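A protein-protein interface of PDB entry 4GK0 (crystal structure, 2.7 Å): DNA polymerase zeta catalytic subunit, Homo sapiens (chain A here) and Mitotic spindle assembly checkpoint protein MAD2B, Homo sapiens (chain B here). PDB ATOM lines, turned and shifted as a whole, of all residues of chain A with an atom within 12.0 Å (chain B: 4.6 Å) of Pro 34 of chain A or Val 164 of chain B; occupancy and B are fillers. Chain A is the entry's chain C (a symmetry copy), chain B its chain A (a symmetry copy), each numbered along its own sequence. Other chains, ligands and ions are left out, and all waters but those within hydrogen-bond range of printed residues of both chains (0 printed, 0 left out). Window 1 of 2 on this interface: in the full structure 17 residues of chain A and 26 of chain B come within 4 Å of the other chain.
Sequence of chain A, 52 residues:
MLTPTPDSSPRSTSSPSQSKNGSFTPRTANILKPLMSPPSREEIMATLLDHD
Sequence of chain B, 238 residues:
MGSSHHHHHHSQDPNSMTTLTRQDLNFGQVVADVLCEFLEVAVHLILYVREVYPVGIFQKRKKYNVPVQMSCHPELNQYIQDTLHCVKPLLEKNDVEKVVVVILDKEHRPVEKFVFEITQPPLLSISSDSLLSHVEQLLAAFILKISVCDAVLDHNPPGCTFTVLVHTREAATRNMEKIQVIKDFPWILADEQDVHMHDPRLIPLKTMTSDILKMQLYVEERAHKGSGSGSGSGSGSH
OH of Tyr 79 of chain B is in hydrogen-bond range of O of Met 36 of chain A, at 2.6 Å. The backbone carbonyl oxygen of Val 166 of chain B is in hydrogen-bond range of the backbone NH of Leu 32 of chain A, 2.8 Å away. O of Pro 186 of chain B lies within hydrogen-bond range of N of Leu 35 of chain A (3.0 Å).
The side-chain hydroxyl (OG1) of Thr 83 of chain B sits at hydrogen-bond distance from the backbone carbonyl oxygen (O) of Tyr 79 of chain B, 2.7 Å away. The backbone carbonyl oxygen (O) of Val 100 of chain B lies within hydrogen-bond range of the backbone NH (N) of Leu 165 of chain B (2.7 Å).
Among the printed residues, pairs that only touch across the chains: Asn 30 of chain A with Val 166 of chain B (3.5 Å), Ile 31 of chain A with Val 166 of chain B (3.2 Å), Leu 32 of chain A with Leu 165 of chain B (3.6 Å), Leu 32 of chain A with Trp 187 of chain B (3.7 Å), Lys 33 of chain A with Leu 165 of chain B (3.4 Å), Lys 33 of chain A with Trp 187 of chain B (3.5 Å), Pro 34 of chain A with Tyr 79 of chain B (3.8 Å), Pro 34 of chain A with Val 164 of chain B (3.3 Å), Pro 34 of chain A with Phe 185 of chain B (3.99 Å), Pro 34 of chain A with Pro 186 of chain B (3.7 Å), Pro 34 of chain A with Trp 187 of chain B (3.4 Å), Ser 37 of chain A with Tyr 79 of chain B (3.4 Å), Pro 38 of chain A with Tyr 79 of chain B (3.3 Å) and Pro 38 of chain A with Phe 162 of chain B (3.2 Å).
Thr 28 of chain A touches none of the printed residues of chain B. Of the printed residues of chain B, Ile 31 of chain A touches Val 166 (3.2 Å). Of the printed residues of chain B, Lys 33 of chain A touches Leu 165 (3.4 Å) and Trp 187 (3.5 Å). Printed residues of chain B within 4 Å of Pro 34 of chain A: Tyr 79, Val 164, Phe 185, Pro 186 and Trp 187. Of the printed residues of chain B, Pro 38 of chain A touches Tyr 79 and Phe 162. Of the printed residues of chain A, Tyr 79 of chain B touches Pro 34, Met 36, Ser 37 and Pro 38. No residue of chain A comes within 4 Å of Val 100 of chain B. No residue of chain A comes within 4 Å of Val 101 of chain B. No residue of chain A comes within 4 Å of Thr 163 of chain B. Val 164 of chain B touches just one residue of chain A: Pro 34. Printed residues of chain A within 4 Å of Val 166 of chain B: Asn 30, Ile 31 and Leu 32. The nearest residue of chain A that does not touch Val 164 of chain B is Lys 33 of chain A (4.03 Å). The nearest printed residue of chain B that does not touch Lys 33 of chain A is Val 164 of chain B (4.03 Å).
Of the 11 printed residues of chain A, 9 touch a printed residue of chain B. Hydrophobic or aromatic side chains of chain A that line the printed part of chain B: Ile 31, Leu 32, Pro 34, Leu 35 and Pro 38. Hydrophobic or aromatic side chains of chain B within 4 Å of the printed part of chain A: Tyr 79, Phe 162, Leu 165, Val 166, Phe 185 and Trp 187.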
ATOM      1  N   THR A  28     -15.126  16.648  -7.279  1.00  0.00           N
ATOM      2  CA  THR A  28     -14.770  15.463  -8.133  1.00  0.00           C
ATOM      3  C   THR A  28     -13.638  15.665  -9.162  1.00  0.00           C
ATOM      4  O   THR A  28     -12.833  16.620  -9.076  1.00  0.00           O
ATOM      5  CB  THR A  28     -15.986  14.841  -8.869  1.00  0.00           C
ATOM      6  OG1 THR A  28     -15.502  13.871  -9.826  1.00  0.00           O
ATOM      7  CG2 THR A  28     -16.830  15.901  -9.594  1.00  0.00           C
ATOM      8  N   ASN A  30     -13.208  16.251 -12.190  1.00  0.00           N
ATOM      9  CA  ASN A  30     -13.233  17.282 -13.189  1.00  0.00           C
ATOM     10  C   ASN A  30     -13.469  18.670 -12.578  1.00  0.00           C
ATOM     11  O   ASN A  30     -13.932  19.564 -13.278  1.00  0.00           O
ATOM     12  CB  ASN A  30     -14.383  16.977 -14.123  1.00  0.00           C
ATOM     13  CG  ASN A  30     -15.697  17.339 -13.500  1.00  0.00           C
ATOM     14  OD1 ASN A  30     -15.953  17.013 -12.339  1.00  0.00           O
ATOM     15  ND2 ASN A  30     -16.520  18.071 -14.240  1.00  0.00           N
ATOM     16  N   ILE A  31     -13.211  18.845 -11.284  1.00  0.00           N
ATOM     17  CA  ILE A  31     -13.175  20.183 -10.723  1.00  0.00           C
ATOM     18  C   ILE A  31     -11.784  20.565 -10.275  1.00  0.00           C
ATOM     19  O   ILE A  31     -11.208  19.900  -9.427  1.00  0.00           O
ATOM     20  CB  ILE A  31     -14.096  20.346  -9.534  1.00  0.00           C
ATOM     21  CG1 ILE A  31     -15.440  19.715  -9.864  1.00  0.00           C
ATOM     22  CG2 ILE A  31     -14.207  21.831  -9.191  1.00  0.00           C
ATOM     23  CD1 ILE A  31     -16.360  19.602  -8.679  1.00  0.00           C
ATOM     24  N   LEU A  32     -11.265  21.651 -10.846  1.00  0.00           N
ATOM     25  CA  LEU A  32      -9.964  22.181 -10.450  1.00  0.00           C
ATOM     26  C   LEU A  32     -10.093  23.445  -9.644  1.00  0.00           C
ATOM     27  O   LEU A  32     -10.986  24.261  -9.874  1.00  0.00           O
ATOM     28  CB  LEU A  32      -9.090  22.413 -11.660  1.00  0.00           C
ATOM     29  CG  LEU A  32      -8.746  21.091 -12.362  1.00  0.00           C
ATOM     30  CD1 LEU A  32      -8.633  21.261 -13.870  1.00  0.00           C
ATOM     31  CD2 LEU A  32      -7.467  20.516 -11.796  1.00  0.00           C
ATOM     32  N   LYS A  33      -9.190  23.616  -8.685  1.00  0.00           N
ATOM     33  CA  LYS A  33      -9.196  24.796  -7.828  1.00  0.00           C
ATOM     34  C   LYS A  33      -7.784  25.176  -7.399  1.00  0.00           C
ATOM     35  O   LYS A  33      -6.953  24.309  -7.126  1.00  0.00           O
ATOM     36  CB  LYS A  33     -10.075  24.560  -6.598  1.00  0.00           C
ATOM     37  CG  LYS A  33      -9.313  24.568  -5.282  1.00  0.00           C
ATOM     38  CD  LYS A  33     -10.259  24.679  -4.097  1.00  0.00           C
ATOM     39  CE  LYS A  33      -9.545  24.379  -2.789  1.00  0.00           C
ATOM     40  NZ  LYS A  33      -9.703  22.956  -2.383  1.00  0.00           N
ATOM     41  N   PRO A  34      -7.517  26.477  -7.342  1.00  0.00           N
ATOM     42  CA  PRO A  34      -6.201  26.977  -6.932  1.00  0.00           C
ATOM     43  C   PRO A  34      -5.836  26.520  -5.523  1.00  0.00           C
ATOM     44  O   PRO A  34      -6.660  26.607  -4.614  1.00  0.00           O
ATOM     45  CB  PRO A  34      -6.384  28.495  -6.961  1.00  0.00           C
ATOM     46  CG  PRO A  34      -7.444  28.720  -7.980  1.00  0.00           C
ATOM     47  CD  PRO A  34      -8.380  27.551  -7.866  1.00  0.00           C
ATOM     48  N   LEU A  35      -4.609  26.037  -5.352  1.00  0.00           N
ATOM     49  CA  LEU A  35      -4.090  25.731  -4.041  1.00  0.00           C
ATOM     50  C   LEU A  35      -4.133  26.907  -3.077  1.00  0.00           C
ATOM     51  O   LEU A  35      -4.534  26.750  -1.939  1.00  0.00           O
ATOM     52  CB  LEU A  35      -2.656  25.249  -4.170  1.00  0.00           C
ATOM     53  CG  LEU A  35      -2.065  24.785  -2.852  1.00  0.00           C
ATOM     54  CD1 LEU A  35      -2.776  23.579  -2.273  1.00  0.00           C
ATOM     55  CD2 LEU A  35      -0.582  24.527  -3.006  1.00  0.00           C
ATOM     56  N   MET A  36      -3.640  28.055  -3.523  1.00  0.00           N
ATOM     57  CA  MET A  36      -3.715  29.332  -2.804  1.00  0.00           C
ATOM     58  C   MET A  36      -5.094  29.930  -2.600  1.00  0.00           C
ATOM     59  O   MET A  36      -5.921  30.054  -3.532  1.00  0.00           O
ATOM     60  CB  MET A  36      -2.965  30.396  -3.564  1.00  0.00           C
ATOM     61  CG  MET A  36      -1.651  30.811  -2.946  1.00  0.00           C
ATOM     62  SD  MET A  36      -0.292  29.787  -3.528  1.00  0.00           S
ATOM     63  CE  MET A  36      -0.047  28.824  -2.028  1.00  0.00           C
ATOM     64  N   SER A  37      -5.278  30.375  -1.366  1.00  0.00           N
ATOM     65  CA  SER A  37      -6.322  31.299  -0.992  1.00  0.00           C
ATOM     66  C   SER A  37      -6.063  32.676  -1.534  1.00  0.00           C
ATOM     67  O   SER A  37      -4.925  33.114  -1.546  1.00  0.00           O
ATOM     68  CB  SER A  37      -6.333  31.396   0.514  1.00  0.00           C
ATOM     69  OG  SER A  37      -7.026  30.276   1.027  1.00  0.00           O
ATOM     70  N   PRO A  38      -7.115  33.392  -1.940  1.00  0.00           N
ATOM     71  CA  PRO A  38      -6.876  34.813  -2.170  1.00  0.00           C
ATOM     72  C   PRO A  38      -6.518  35.538  -0.874  1.00  0.00           C
ATOM     73  O   PRO A  38      -6.859  35.049   0.185  1.00  0.00           O
ATOM     74  CB  PRO A  38      -8.212  35.310  -2.725  1.00  0.00           C
ATOM     75  CG  PRO A  38      -9.204  34.421  -2.132  1.00  0.00           C
ATOM     76  CD  PRO A  38      -8.551  33.079  -1.907  1.00  0.00           C
ATOM     77  N   PRO A  39      -5.829  36.697  -0.957  1.00  0.00           N
ATOM     78  CA  PRO A  39      -5.589  37.494   0.243  1.00  0.00           C
ATOM     79  C   PRO A  39      -6.880  37.812   0.972  1.00  0.00           C
ATOM     80  O   PRO A  39      -7.850  38.254   0.345  1.00  0.00           O
ATOM     81  CB  PRO A  39      -4.990  38.776  -0.290  1.00  0.00           C
ATOM     82  CG  PRO A  39      -5.296  38.806  -1.736  1.00  0.00           C
ATOM     83  CD  PRO A  39      -5.329  37.375  -2.159  1.00  0.00           C
ATOM     84  N   TYR B  79      -3.699  37.663  -7.909  1.00  0.00           N
ATOM     85  CA  TYR B  79      -4.415  36.422  -7.707  1.00  0.00           C
ATOM     86  C   TYR B  79      -5.455  36.126  -8.808  1.00  0.00           C
ATOM     87  O   TYR B  79      -5.486  35.048  -9.425  1.00  0.00           O
ATOM     88  CB  TYR B  79      -5.109  36.468  -6.376  1.00  0.00           C
ATOM     89  CG  TYR B  79      -5.757  35.161  -6.027  1.00  0.00           C
ATOM     90  CD1 TYR B  79      -5.096  34.241  -5.259  1.00  0.00           C
ATOM     91  CD2 TYR B  79      -7.032  34.843  -6.486  1.00  0.00           C
ATOM     92  CE1 TYR B  79      -5.674  33.035  -4.938  1.00  0.00           C
ATOM     93  CE2 TYR B  79      -7.620  33.642  -6.172  1.00  0.00           C
ATOM     94  CZ  TYR B  79      -6.934  32.744  -5.394  1.00  0.00           C
ATOM     95  OH  TYR B  79      -7.488  31.543  -5.039  1.00  0.00           O
ATOM     96  N   THR B  83      -5.124  33.337 -11.734  1.00  0.00           N
ATOM     97  CA  THR B  83      -6.202  32.351 -11.871  1.00  0.00           C
ATOM     98  C   THR B  83      -6.644  32.244 -13.327  1.00  0.00           C
ATOM     99  O   THR B  83      -6.604  31.187 -13.924  1.00  0.00           O
ATOM    100  CB  THR B  83      -7.370  32.765 -10.994  1.00  0.00           C
ATOM    101  OG1 THR B  83      -6.929  32.788  -9.631  1.00  0.00           O
ATOM    102  CG2 THR B  83      -8.540  31.820 -11.157  1.00  0.00           C
ATOM    103  N   VAL B  99     -16.946  28.004 -15.079  1.00  0.00           N
ATOM    104  CA  VAL B  99     -16.103  28.667 -14.126  1.00  0.00           C
ATOM    105  C   VAL B  99     -17.033  29.153 -13.007  1.00  0.00           C
ATOM    106  O   VAL B  99     -18.061  29.760 -13.268  1.00  0.00           O
ATOM    107  CB  VAL B  99     -15.316  29.809 -14.797  1.00  0.00           C
ATOM    108  CG1 VAL B  99     -14.541  30.605 -13.779  1.00  0.00           C
ATOM    109  CG2 VAL B  99     -14.362  29.246 -15.798  1.00  0.00           C
ATOM    110  N   VAL B 100     -16.670  28.882 -11.763  1.00  0.00           N
ATOM    111  CA  VAL B 100     -17.530  29.214 -10.628  1.00  0.00           C
ATOM    112  C   VAL B 100     -16.791  30.073  -9.592  1.00  0.00           C
ATOM    113  O   VAL B 100     -15.725  29.690  -9.081  1.00  0.00           O
ATOM    114  CB  VAL B 100     -18.129  27.978  -9.955  1.00  0.00           C
ATOM    115  CG1 VAL B 100     -18.987  28.420  -8.790  1.00  0.00           C
ATOM    116  CG2 VAL B 100     -19.021  27.193 -10.933  1.00  0.00           C
ATOM    117  N   VAL B 101     -17.335  31.259  -9.321  1.00  0.00           N
ATOM    118  CA  VAL B 101     -16.844  32.079  -8.219  1.00  0.00           C
ATOM    119  C   VAL B 101     -17.664  31.675  -6.995  1.00  0.00           C
ATOM    120  O   VAL B 101     -18.866  31.887  -6.939  1.00  0.00           O
ATOM    121  CB  VAL B 101     -16.993  33.588  -8.492  1.00  0.00           C
ATOM    122  CG1 VAL B 101     -16.461  34.440  -7.349  1.00  0.00           C
ATOM    123  CG2 VAL B 101     -16.272  33.924  -9.779  1.00  0.00           C
ATOM    124  N   PHE B 162     -13.607  34.226  -0.783  1.00  0.00           N
ATOM    125  CA  PHE B 162     -13.941  33.611  -2.047  1.00  0.00           C
ATOM    126  C   PHE B 162     -12.898  32.624  -2.518  1.00  0.00           C
ATOM    127  O   PHE B 162     -11.780  32.601  -2.030  1.00  0.00           O
ATOM    128  CB  PHE B 162     -14.253  34.681  -3.119  1.00  0.00           C
ATOM    129  CG  PHE B 162     -13.075  35.158  -3.919  1.00  0.00           C
ATOM    130  CD1 PHE B 162     -12.245  36.163  -3.446  1.00  0.00           C
ATOM    131  CD2 PHE B 162     -12.837  34.665  -5.189  1.00  0.00           C
ATOM    132  CE1 PHE B 162     -11.189  36.670  -4.201  1.00  0.00           C
ATOM    133  CE2 PHE B 162     -11.781  35.165  -5.962  1.00  0.00           C
ATOM    134  CZ  PHE B 162     -10.952  36.175  -5.466  1.00  0.00           C
ATOM    135  N   THR B 163     -13.314  31.809  -3.481  1.00  0.00           N
ATOM    136  CA  THR B 163     -12.499  30.855  -4.191  1.00  0.00           C
ATOM    137  C   THR B 163     -13.113  30.808  -5.588  1.00  0.00           C
ATOM    138  O   THR B 163     -14.272  31.111  -5.712  1.00  0.00           O
ATOM    139  CB  THR B 163     -12.519  29.436  -3.559  1.00  0.00           C
ATOM    140  OG1 THR B 163     -12.099  28.468  -4.530  1.00  0.00           O
ATOM    141  CG2 THR B 163     -13.878  28.990  -3.216  1.00  0.00           C
ATOM    142  N   VAL B 164     -12.322  30.453  -6.607  1.00  0.00           N
ATOM    143  CA  VAL B 164     -12.783  30.148  -7.959  1.00  0.00           C
ATOM    144  C   VAL B 164     -12.625  28.656  -8.249  1.00  0.00           C
ATOM    145  O   VAL B 164     -11.648  28.049  -7.864  1.00  0.00           O
ATOM    146  CB  VAL B 164     -11.953  30.882  -9.003  1.00  0.00           C
ATOM    147  CG1 VAL B 164     -12.378  30.503 -10.412  1.00  0.00           C
ATOM    148  CG2 VAL B 164     -12.061  32.377  -8.814  1.00  0.00           C
ATOM    149  N   LEU B 165     -13.602  28.064  -8.922  1.00  0.00           N
ATOM    150  CA  LEU B 165     -13.560  26.648  -9.279  1.00  0.00           C
ATOM    151  C   LEU B 165     -13.798  26.468 -10.781  1.00  0.00           C
ATOM    152  O   LEU B 165     -14.614  27.151 -11.364  1.00  0.00           O
ATOM    153  CB  LEU B 165     -14.623  25.881  -8.508  1.00  0.00           C
ATOM    154  CG  LEU B 165     -14.570  25.717  -6.984  1.00  0.00           C
ATOM    155  CD1 LEU B 165     -15.825  25.045  -6.468  1.00  0.00           C
ATOM    156  CD2 LEU B 165     -13.431  24.839  -6.526  1.00  0.00           C
ATOM    157  N   VAL B 166     -13.048  25.578 -11.412  1.00  0.00           N
ATOM    158  CA  VAL B 166     -13.221  25.259 -12.831  1.00  0.00           C
ATOM    159  C   VAL B 166     -13.794  23.849 -12.960  1.00  0.00           C
ATOM    160  O   VAL B 166     -13.196  22.908 -12.445  1.00  0.00           O
ATOM    161  CB  VAL B 166     -11.883  25.294 -13.505  1.00  0.00           C
ATOM    162  CG1 VAL B 166     -11.955  24.843 -14.927  1.00  0.00           C
ATOM    163  CG2 VAL B 166     -11.346  26.685 -13.455  1.00  0.00           C
ATOM    164  N   PHE B 185       1.845  29.352  -8.837  1.00  0.00           N
ATOM    165  CA  PHE B 185       0.394  29.292  -8.732  1.00  0.00           C
ATOM    166  C   PHE B 185      -0.218  27.958  -9.191  1.00  0.00           C
ATOM    167  O   PHE B 185      -0.904  27.900 -10.195  1.00  0.00           O
ATOM    168  CB  PHE B 185      -0.220  30.476  -9.504  1.00  0.00           C
ATOM    169  CG  PHE B 185      -1.596  30.862  -9.030  1.00  0.00           C
ATOM    170  CD1 PHE B 185      -1.753  31.685  -7.946  1.00  0.00           C
ATOM    171  CD2 PHE B 185      -2.725  30.395  -9.676  1.00  0.00           C
ATOM    172  CE1 PHE B 185      -2.999  32.022  -7.488  1.00  0.00           C
ATOM    173  CE2 PHE B 185      -3.985  30.736  -9.225  1.00  0.00           C
ATOM    174  CZ  PHE B 185      -4.116  31.559  -8.128  1.00  0.00           C
ATOM    175  N   PRO B 186      -0.027  26.887  -8.430  1.00  0.00           N
ATOM    176  CA  PRO B 186      -0.582  25.575  -8.678  1.00  0.00           C
ATOM    177  C   PRO B 186      -2.047  25.339  -8.366  1.00  0.00           C
ATOM    178  O   PRO B 186      -2.650  26.066  -7.587  1.00  0.00           O
ATOM    179  CB  PRO B 186       0.207  24.667  -7.739  1.00  0.00           C
ATOM    180  CG  PRO B 186       1.184  25.528  -7.031  1.00  0.00           C
ATOM    181  CD  PRO B 186       0.737  26.930  -7.187  1.00  0.00           C
ATOM    182  N   TRP B 187      -2.559  24.232  -8.891  1.00  0.00           N
ATOM    183  CA  TRP B 187      -3.964  23.886  -8.879  1.00  0.00           C
ATOM    184  C   TRP B 187      -4.089  22.482  -8.323  1.00  0.00           C
ATOM    185  O   TRP B 187      -3.211  21.660  -8.483  1.00  0.00           O
ATOM    186  CB  TRP B 187      -4.580  23.932 -10.286  1.00  0.00           C
ATOM    187  CG  TRP B 187      -4.769  25.297 -10.819  1.00  0.00           C
ATOM    188  CD1 TRP B 187      -3.796  26.153 -11.198  1.00  0.00           C
ATOM    189  CD2 TRP B 187      -6.002  25.993 -11.032  1.00  0.00           C
ATOM    190  NE1 TRP B 187      -4.333  27.328 -11.655  1.00  0.00           N
ATOM    191  CE2 TRP B 187      -5.693  27.245 -11.559  1.00  0.00           C
ATOM    192  CE3 TRP B 187      -7.341  25.674 -10.841  1.00  0.00           C
ATOM    193  CZ2 TRP B 187      -6.669  28.179 -11.863  1.00  0.00           C
ATOM    194  CZ3 TRP B 187      -8.303  26.606 -11.153  1.00  0.00           C
ATOM    195  CH2 TRP B 187      -7.963  27.838 -11.649  1.00  0.00           C
